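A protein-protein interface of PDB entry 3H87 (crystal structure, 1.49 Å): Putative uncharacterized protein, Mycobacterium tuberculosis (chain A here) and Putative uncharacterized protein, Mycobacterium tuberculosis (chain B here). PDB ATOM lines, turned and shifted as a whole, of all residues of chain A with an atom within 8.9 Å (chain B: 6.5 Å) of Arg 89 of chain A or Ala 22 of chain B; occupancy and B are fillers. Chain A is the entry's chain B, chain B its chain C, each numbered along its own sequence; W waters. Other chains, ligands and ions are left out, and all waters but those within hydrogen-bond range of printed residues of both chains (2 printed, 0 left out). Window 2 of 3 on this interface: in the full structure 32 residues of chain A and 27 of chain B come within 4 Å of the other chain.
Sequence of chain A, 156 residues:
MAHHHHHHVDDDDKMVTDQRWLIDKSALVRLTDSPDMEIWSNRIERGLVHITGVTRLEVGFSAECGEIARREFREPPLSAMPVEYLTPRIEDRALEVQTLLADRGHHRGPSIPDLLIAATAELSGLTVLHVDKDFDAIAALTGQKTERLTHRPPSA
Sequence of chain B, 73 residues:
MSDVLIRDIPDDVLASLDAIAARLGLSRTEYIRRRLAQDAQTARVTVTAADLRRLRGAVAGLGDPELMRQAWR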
ATOM      1  N   LEU A  86      11.334  27.568  32.710  1.00  0.00           N
ATOM      2  CA  LEU A  86      12.020  26.314  32.981  1.00  0.00           C
ATOM      3  C   LEU A  86      11.126  25.093  32.917  1.00  0.00           C
ATOM      4  O   LEU A  86       9.884  25.185  32.988  1.00  0.00           O
ATOM      5  CB  LEU A  86      12.717  26.374  34.356  1.00  0.00           C
ATOM      6  CG  LEU A  86      13.924  27.327  34.428  1.00  0.00           C
ATOM      7  CD1 LEU A  86      14.283  27.759  35.848  1.00  0.00           C
ATOM      8  CD2 LEU A  86      15.119  26.689  33.730  1.00  0.00           C
ATOM      9  N   THR A  87      11.740  23.926  32.765  1.00  0.00           N
ATOM     10  CA  THR A  87      11.077  22.616  32.881  1.00  0.00           C
ATOM     11  C   THR A  87      11.948  21.725  33.774  1.00  0.00           C
ATOM     12  O   THR A  87      13.133  22.032  33.975  1.00  0.00           O
ATOM     13  CB  THR A  87      10.880  21.894  31.543  1.00  0.00           C
ATOM     14  OG1 THR A  87      12.173  21.401  31.084  1.00  0.00           O
ATOM     15  CG2 THR A  87      10.249  22.770  30.505  1.00  0.00           C
ATOM     16  N   PRO A  88      11.433  20.592  34.289  1.00  0.00           N
ATOM     17  CA  PRO A  88      12.251  19.796  35.179  1.00  0.00           C
ATOM     18  C   PRO A  88      13.517  19.239  34.523  1.00  0.00           C
ATOM     19  O   PRO A  88      14.578  19.174  35.129  1.00  0.00           O
ATOM     20  CB  PRO A  88      11.290  18.665  35.637  1.00  0.00           C
ATOM     21  CG  PRO A  88       9.940  19.332  35.628  1.00  0.00           C
ATOM     22  CD  PRO A  88       9.994  20.229  34.403  1.00  0.00           C
ATOM     23  N   ARG A  89      13.454  18.864  33.243  1.00  0.00           N
ATOM     24  CA  ARG A  89      14.596  18.404  32.527  1.00  0.00           C
ATOM     25  C   ARG A  89      15.656  19.481  32.333  1.00  0.00           C
ATOM     26  O   ARG A  89      16.859  19.191  32.355  1.00  0.00           O
ATOM     27  CB  ARG A  89      14.134  17.882  31.175  1.00  0.00           C
ATOM     28  CG  ARG A  89      15.112  17.202  30.373  1.00  0.00           C
ATOM     29  CD  ARG A  89      15.297  15.720  30.715  1.00  0.00           C
ATOM     30  NE  ARG A  89      14.063  14.946  30.552  1.00  0.00           N
ATOM     31  CZ  ARG A  89      13.755  14.136  29.535  1.00  0.00           C
ATOM     32  NH1 ARG A  89      14.572  13.956  28.479  1.00  0.00           N
ATOM     33  NH2 ARG A  89      12.588  13.492  29.577  1.00  0.00           N
ATOM     34  N   ILE A  90      15.256  20.757  32.140  1.00  0.00           N
ATOM     35  CA  ILE A  90      16.231  21.850  32.051  1.00  0.00           C
ATOM     36  C   ILE A  90      16.932  22.008  33.412  1.00  0.00           C
ATOM     37  O   ILE A  90      18.163  22.145  33.491  1.00  0.00           O
ATOM     38  CB  ILE A  90      15.585  23.154  31.593  1.00  0.00           C
ATOM     39  CG1 ILE A  90      15.062  23.082  30.134  1.00  0.00           C
ATOM     40  CG2 ILE A  90      16.580  24.297  31.729  1.00  0.00           C
ATOM     41  CD1 ILE A  90      14.108  24.269  29.751  1.00  0.00           C
ATOM     42  N   GLU A  91      16.146  22.024  34.507  1.00  0.00           N
ATOM     43  CA  GLU A  91      16.766  22.179  35.849  1.00  0.00           C
ATOM     44  C   GLU A  91      17.747  21.034  36.125  1.00  0.00           C
ATOM     45  O   GLU A  91      18.840  21.262  36.677  1.00  0.00           O
ATOM     46  CB  GLU A  91      15.673  22.238  36.932  1.00  0.00           C
ATOM     47  CG  GLU A  91      14.804  23.513  36.844  1.00  0.00           C
ATOM     48  CD  GLU A  91      13.965  23.778  38.057  1.00  0.00           C
ATOM     49  OE1 GLU A  91      14.528  23.892  39.162  1.00  0.00           O
ATOM     50  OE2 GLU A  91      12.717  23.853  37.954  1.00  0.00           O
ATOM     51  N   ASP A  92      17.370  19.797  35.802  1.00  0.00           N
ATOM     52  CA  ASP A  92      18.271  18.684  36.010  1.00  0.00           C
ATOM     53  C   ASP A  92      19.532  18.802  35.116  1.00  0.00           C
ATOM     54  O   ASP A  92      20.637  18.415  35.542  1.00  0.00           O
ATOM     55  CB  ASP A  92      17.538  17.358  35.700  1.00  0.00           C
ATOM     56  CG  ASP A  92      16.522  16.946  36.770  1.00  0.00           C
ATOM     57  OD1 ASP A  92      16.520  17.481  37.898  1.00  0.00           O
ATOM     58  OD2 ASP A  92      15.701  16.029  36.459  1.00  0.00           O
ATOM     59  N   ARG A  93      19.377  19.247  33.873  1.00  0.00           N
ATOM     60  CA  ARG A  93      20.518  19.437  32.985  1.00  0.00           C
ATOM     61  C   ARG A  93      21.501  20.452  33.511  1.00  0.00           C
ATOM     62  O   ARG A  93      22.704  20.259  33.428  1.00  0.00           O
ATOM     63  CB  ARG A  93      20.041  19.847  31.577  1.00  0.00           C
ATOM     64  CG  ARG A  93      21.167  19.994  30.543  1.00  0.00           C
ATOM     65  CD  ARG A  93      22.078  18.766  30.384  1.00  0.00           C
ATOM     66  NE  ARG A  93      23.028  18.998  29.307  1.00  0.00           N
ATOM     67  CZ  ARG A  93      24.071  18.234  29.078  1.00  0.00           C
ATOM     68  NH1 ARG A  93      24.314  17.220  29.879  1.00  0.00           N
ATOM     69  NH2 ARG A  93      24.856  18.480  28.052  1.00  0.00           N
ATOM     70  N   ALA A  94      20.992  21.574  34.028  1.00  0.00           N
ATOM     71  CA  ALA A  94      21.884  22.565  34.629  1.00  0.00           C
ATOM     72  C   ALA A  94      22.740  21.951  35.738  1.00  0.00           C
ATOM     73  O   ALA A  94      23.952  22.226  35.853  1.00  0.00           O
ATOM     74  CB  ALA A  94      21.081  23.773  35.167  1.00  0.00           C
ATOM     75  N   LEU A  95      22.141  21.097  36.560  1.00  0.00           N
ATOM     76  CA  LEU A  95      22.877  20.430  37.630  1.00  0.00           C
ATOM     77  C   LEU A  95      23.895  19.432  37.103  1.00  0.00           C
ATOM     78  O   LEU A  95      25.016  19.332  37.646  1.00  0.00           O
ATOM     79  CB  LEU A  95      21.906  19.752  38.632  1.00  0.00           C
ATOM     80  CG  LEU A  95      22.500  19.205  39.935  1.00  0.00           C
ATOM     81  CD1 LEU A  95      23.018  20.315  40.843  1.00  0.00           C
ATOM     82  CD2 LEU A  95      21.449  18.382  40.750  1.00  0.00           C
ATOM     83  N   GLU A  96      23.516  18.672  36.086  1.00  0.00           N
ATOM     84  CA  GLU A  96      24.470  17.762  35.450  1.00  0.00           C
ATOM     85  C   GLU A  96      25.668  18.511  34.880  1.00  0.00           C
ATOM     86  O   GLU A  96      26.830  18.093  35.054  1.00  0.00           O
ATOM     87  CB  GLU A  96      23.767  16.981  34.327  1.00  0.00           C
ATOM     88  CG  GLU A  96      24.620  15.948  33.692  1.00  0.00           C
ATOM     89  CD  GLU A  96      24.030  15.269  32.460  1.00  0.00           C
ATOM     90  OE1 GLU A  96      22.973  15.703  31.902  1.00  0.00           O
ATOM     91  OE2 GLU A  96      24.643  14.235  32.078  1.00  0.00           O
ATOM     92  N   VAL A  97      25.410  19.584  34.139  1.00  0.00           N
ATOM     93  CA  VAL A  97      26.514  20.396  33.580  1.00  0.00           C
ATOM     94  C   VAL A  97      27.401  20.954  34.695  1.00  0.00           C
ATOM     95  O   VAL A  97      28.632  20.893  34.605  1.00  0.00           O
ATOM     96  CB  VAL A  97      25.963  21.531  32.669  1.00  0.00           C
ATOM     97  CG1 VAL A  97      27.052  22.514  32.234  1.00  0.00           C
ATOM     98  CG2 VAL A  97      25.306  20.915  31.426  1.00  0.00           C
ATOM     99  N   LEU A 115      24.222  28.748  34.138  1.00  0.00           N
ATOM    100  CA  LEU A 115      23.865  27.327  33.912  1.00  0.00           C
ATOM    101  C   LEU A 115      22.404  27.147  33.476  1.00  0.00           C
ATOM    102  O   LEU A 115      22.079  26.325  32.598  1.00  0.00           O
ATOM    103  CB  LEU A 115      24.144  26.502  35.167  1.00  0.00           C
ATOM    104  CG  LEU A 115      25.595  26.374  35.574  1.00  0.00           C
ATOM    105  CD1 LEU A 115      25.758  26.003  37.053  1.00  0.00           C
ATOM    106  CD2 LEU A 115      26.282  25.350  34.649  1.00  0.00           C
ATOM    107  N   LEU A 116      21.493  27.900  34.099  1.00  0.00           N
ATOM    108  CA  LEU A 116      20.073  27.798  33.756  1.00  0.00           C
ATOM    109  C   LEU A 116      19.778  28.358  32.365  1.00  0.00           C
ATOM    110  O   LEU A 116      18.980  27.769  31.619  1.00  0.00           O
ATOM    111  CB  LEU A 116      19.239  28.511  34.849  1.00  0.00           C
ATOM    112  CG  LEU A 116      19.154  27.808  36.205  1.00  0.00           C
ATOM    113  CD1 LEU A 116      18.512  28.708  37.306  1.00  0.00           C
ATOM    114  CD2 LEU A 116      18.424  26.455  36.126  1.00  0.00           C
ATOM    115  N   ALA A 119      21.277  25.838  29.810  1.00  0.00           N
ATOM    116  CA  ALA A 119      20.518  24.602  29.664  1.00  0.00           C
ATOM    117  C   ALA A 119      19.186  24.837  28.969  1.00  0.00           C
ATOM    118  O   ALA A 119      18.721  23.986  28.173  1.00  0.00           O
ATOM    119  CB  ALA A 119      20.314  23.967  31.050  1.00  0.00           C
ATOM    120  N   THR A 120      18.545  25.995  29.227  1.00  0.00           N
ATOM    121  CA  THR A 120      17.323  26.321  28.525  1.00  0.00           C
ATOM    122  C   THR A 120      17.571  26.389  27.014  1.00  0.00           C
ATOM    123  O   THR A 120      16.830  25.844  26.200  1.00  0.00           O
ATOM    124  CB  THR A 120      16.755  27.679  29.030  1.00  0.00           C
ATOM    125  OG1 THR A 120      16.437  27.592  30.433  1.00  0.00           O
ATOM    126  CG2 THR A 120      15.464  28.035  28.258  1.00  0.00           C
ATOM    127  N   GLU A 122      20.061  25.108  25.275  1.00  0.00           N
ATOM    128  CA  GLU A 122      20.495  23.789  24.754  1.00  0.00           C
ATOM    129  C   GLU A 122      19.298  22.921  24.432  1.00  0.00           C
ATOM    130  O   GLU A 122      19.198  22.374  23.330  1.00  0.00           O
ATOM    131  CB  GLU A 122      21.377  23.081  25.801  1.00  0.00           C
ATOM    132  CG  GLU A 122      21.990  21.755  25.335  1.00  0.00           C
ATOM    133  CD  GLU A 122      22.721  20.990  26.419  1.00  0.00           C
ATOM    134  OE1 GLU A 122      22.705  21.326  27.646  1.00  0.00           O
ATOM    135  OE2 GLU A 122      23.431  19.976  26.022  1.00  0.00           O
ATOM    136  N   LEU A 123      18.361  22.788  25.371  1.00  0.00           N
ATOM    137  CA  LEU A 123      17.236  21.848  25.174  1.00  0.00           C
ATOM    138  C   LEU A 123      16.137  22.429  24.295  1.00  0.00           C
ATOM    139  O   LEU A 123      15.299  21.707  23.778  1.00  0.00           O
ATOM    140  CB  LEU A 123      16.693  21.394  26.528  1.00  0.00           C
ATOM    141  CG  LEU A 123      17.608  20.546  27.388  1.00  0.00           C
ATOM    142  CD1 LEU A 123      16.884  19.954  28.601  1.00  0.00           C
ATOM    143  CD2 LEU A 123      18.447  19.487  26.617  1.00  0.00           C
ATOM    144  N   LEU B  17       6.676  17.733  17.293  1.00  0.00           N
ATOM    145  CA  LEU B  17       6.124  18.134  18.586  1.00  0.00           C
ATOM    146  C   LEU B  17       6.512  17.136  19.673  1.00  0.00           C
ATOM    147  O   LEU B  17       6.940  17.524  20.761  1.00  0.00           O
ATOM    148  CB  LEU B  17       4.596  18.274  18.528  1.00  0.00           C
ATOM    149  CG  LEU B  17       4.037  19.461  17.760  1.00  0.00           C
ATOM    150  CD1 LEU B  17       2.540  19.279  17.517  1.00  0.00           C
ATOM    151  CD2 LEU B  17       4.316  20.751  18.521  1.00  0.00           C
ATOM    152  N   ASP B  18       6.345  15.854  19.384  1.00  0.00           N
ATOM    153  CA  ASP B  18       6.759  14.822  20.313  1.00  0.00           C
ATOM    154  C   ASP B  18       8.254  14.875  20.639  1.00  0.00           C
ATOM    155  O   ASP B  18       8.618  14.639  21.778  1.00  0.00           O
ATOM    156  CB  ASP B  18       6.370  13.445  19.767  1.00  0.00           C
ATOM    157  CG  ASP B  18       4.878  13.164  19.889  1.00  0.00           C
ATOM    158  OD1 ASP B  18       4.204  13.845  20.688  1.00  0.00           O
ATOM    159  OD2 ASP B  18       4.373  12.241  19.197  1.00  0.00           O
ATOM    160  N   ALA B  19       9.129  15.154  19.672  1.00  0.00           N
ATOM    161  CA  ALA B  19      10.572  15.193  19.979  1.00  0.00           C
ATOM    162  C   ALA B  19      10.895  16.380  20.878  1.00  0.00           C
ATOM    163  O   ALA B  19      11.744  16.283  21.770  1.00  0.00           O
ATOM    164  CB  ALA B  19      11.419  15.242  18.718  1.00  0.00           C
ATOM    165  N   ILE B  20      10.241  17.505  20.634  1.00  0.00           N
ATOM    166  CA  ILE B  20      10.494  18.691  21.435  1.00  0.00           C
ATOM    167  C   ILE B  20      10.034  18.482  22.876  1.00  0.00           C
ATOM    168  O   ILE B  20      10.751  18.774  23.833  1.00  0.00           O
ATOM    169  CB  ILE B  20       9.727  19.900  20.821  1.00  0.00           C
ATOM    170  CG1 ILE B  20      10.211  20.190  19.385  1.00  0.00           C
ATOM    171  CG2 ILE B  20       9.873  21.126  21.695  1.00  0.00           C
ATOM    172  CD1 ILE B  20       9.262  21.108  18.536  1.00  0.00           C
ATOM    173  N   ALA B  21       8.807  18.012  23.034  1.00  0.00           N
ATOM    174  CA  ALA B  21       8.220  17.734  24.347  1.00  0.00           C
ATOM    175  C   ALA B  21       9.109  16.772  25.114  1.00  0.00           C
ATOM    176  O   ALA B  21       9.432  17.007  26.278  1.00  0.00           O
ATOM    177  CB  ALA B  21       6.770  17.183  24.216  1.00  0.00           C
ATOM    178  N   ALA B  22       9.553  15.697  24.458  1.00  0.00           N
ATOM    179  CA  ALA B  22      10.399  14.699  25.112  1.00  0.00           C
ATOM    180  C   ALA B  22      11.706  15.332  25.608  1.00  0.00           C
ATOM    181  O   ALA B  22      12.174  15.055  26.740  1.00  0.00           O
ATOM    182  CB  ALA B  22      10.689  13.522  24.149  1.00  0.00           C
ATOM    183  N   ARG B  23      12.325  16.167  24.783  1.00  0.00           N
ATOM    184  CA  ARG B  23      13.600  16.764  25.121  1.00  0.00           C
ATOM    185  C   ARG B  23      13.470  17.682  26.344  1.00  0.00           C
ATOM    186  O   ARG B  23      14.423  17.810  27.153  1.00  0.00           O
ATOM    187  CB  ARG B  23      14.129  17.525  23.906  1.00  0.00           C
ATOM    188  CG  ARG B  23      15.505  18.090  24.053  1.00  0.00           C
ATOM    189  CD  ARG B  23      16.112  18.320  22.677  1.00  0.00           C
ATOM    190  NE  ARG B  23      17.354  19.077  22.747  1.00  0.00           N
ATOM    191  CZ  ARG B  23      18.550  18.549  23.002  1.00  0.00           C
ATOM    192  NH1 ARG B  23      18.693  17.233  23.176  1.00  0.00           N
ATOM    193  NH2 ARG B  23      19.626  19.321  23.053  1.00  0.00           N
ATOM    194  N   LEU B  24      12.300  18.303  26.501  1.00  0.00           N
ATOM    195  CA  LEU B  24      12.043  19.181  27.640  1.00  0.00           C
ATOM    196  C   LEU B  24      11.449  18.481  28.878  1.00  0.00           C
ATOM    197  O   LEU B  24      11.375  19.090  29.980  1.00  0.00           O
ATOM    198  CB  LEU B  24      11.100  20.315  27.218  1.00  0.00           C
ATOM    199  CG  LEU B  24      11.613  21.294  26.166  1.00  0.00           C
ATOM    200  CD1 LEU B  24      10.443  22.169  25.603  1.00  0.00           C
ATOM    201  CD2 LEU B  24      12.689  22.170  26.738  1.00  0.00           C
ATOM    202  N   GLY B  25      11.050  17.213  28.736  1.00  0.00           N
ATOM    203  CA  GLY B  25      10.371  16.520  29.836  1.00  0.00           C
ATOM    204  C   GLY B  25       8.937  16.971  30.090  1.00  0.00           C
ATOM    205  O   GLY B  25       8.503  17.131  31.285  1.00  0.00           O
ATOM    206  N   LEU B  26       8.260  17.361  29.002  1.00  0.00           N
ATOM    207  CA  LEU B  26       6.874  17.744  29.081  1.00  0.00           C
ATOM    208  C   LEU B  26       6.029  16.754  28.295  1.00  0.00           C
ATOM    209  O   LEU B  26       6.500  16.137  27.327  1.00  0.00           O
ATOM    210  CB  LEU B  26       6.650  19.133  28.489  1.00  0.00           C
ATOM    211  CG  LEU B  26       7.349  20.309  29.138  1.00  0.00           C
ATOM    212  CD1 LEU B  26       7.085  21.603  28.363  1.00  0.00           C
ATOM    213  CD2 LEU B  26       6.986  20.465  30.599  1.00  0.00           C
ATOM    214  N   SER B  27       4.782  16.637  28.689  1.00  0.00           N
ATOM    215  CA  SER B  27       3.853  15.934  27.850  1.00  0.00           C
ATOM    216  C   SER B  27       3.587  16.715  26.559  1.00  0.00           C
ATOM    217  O   SER B  27       3.804  17.945  26.489  1.00  0.00           O
ATOM    218  CB  SER B  27       2.532  15.701  28.582  1.00  0.00           C
ATOM    219  OG  SER B  27       1.780  16.887  28.688  1.00  0.00           O
HETATM  220  O   HOH W   1      16.579  16.129  27.422  1.00  0.00           O
HETATM  221  O   HOH W   2      10.601  18.218  32.419  1.00  0.00           O
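Water W2 lies within hydrogen-bond range of the backbone carbonyl oxygen (O) of Gly 25 of chain B (2.6 Å), the backbone carbonyl oxygen (O) of Leu 24 of chain B (2.7 Å) and the backbone NH (N) of Arg 89 of chain A (3.0 Å).
Water W1 lies within hydrogen-bond range of the backbone carbonyl oxygen of Arg 23 of chain B (2.7 Å) and the guanidinium group of Arg 89 of chain A (3.1 Å).
Among the printed residues, merely in contact across the chains: Thr 87 of chain A with Leu 26 of chain B (3.995 Å), Arg 89 of chain A with Arg 23 of chain B (3.3 Å), Arg 89 of chain A with Leu 24 of chain B (3.2 Å), Arg 89 of chain A with Gly 25 of chain B (3.8 Å), Ile 90 of chain A with Leu 24 of chain B (3.9 Å) and Leu 123 of chain A with Leu 24 of chain B (3.97 Å).
Of the printed residues of chain B, Arg 89 of chain A touches Ala 22 (3.2 Å), Arg 23 (3.3 Å), Leu 24 (3.2 Å) and Gly 25 (3.8 Å).
Ala 22 of chain B touches just one residue of chain A: Arg 89 (3.2 Å).
Printed residues of chain B within 4 Å of Ile 90 of chain A: Leu 24 (3.9 Å).
Of the printed residues of chain B, Thr 87 of chain A touches Leu 24 (2.7 Å) and Leu 26 (3.995 Å).
Of the printed residues of chain A, Gly 25 of chain B touches Arg 89.
Thr 120 of chain A touches none of the printed residues of chain B.
OG1 of Thr 87 of chain A sits at hydrogen-bond distance from N of Ile 90 of chain A (3.3 Å).
NE of Arg 93 of chain A lies within salt-bridge range of OE1 of Glu 122 of chain A (2.9 Å).
N of Leu 26 of chain B sits at hydrogen-bond distance from O of Ala 21 of chain B.
Of the 11 printed residues of chain B, 5 touch a printed residue of chain A.
Printed residues of chain B that touch a printed residue of chain A: Ala 22, Arg 23, Leu 24, Gly 25 and Leu 26.
Hydrophobic or aromatic side chains of chain B that line the printed part of chain A: Leu 24 and Leu 26.
Hydrophobic or aromatic side chains of chain A that line the printed part of chain B: Ile 90 and Leu 123.
The side-chain hydroxyl of Thr 87 of chain A lies within hydrogen-bond range of the backbone carbonyl oxygen of Leu 24 of chain B (2.7 Å).
The guanidinium group of Arg 89 of chain A is in hydrogen-bond range of the backbone carbonyl oxygen of Ala 22 of chain B, 3.2 Å away.
The backbone carbonyl oxygen of Glu 122 of chain A sits at hydrogen-bond distance from the guanidinium group of Arg 23 of chain B (3.1 Å).
The backbone carbonyl oxygen (O) of Leu 123 of chain A lies within hydrogen-bond range of the guanidinium group (NE) of Arg 23 of chain B, at 3.5 Å.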
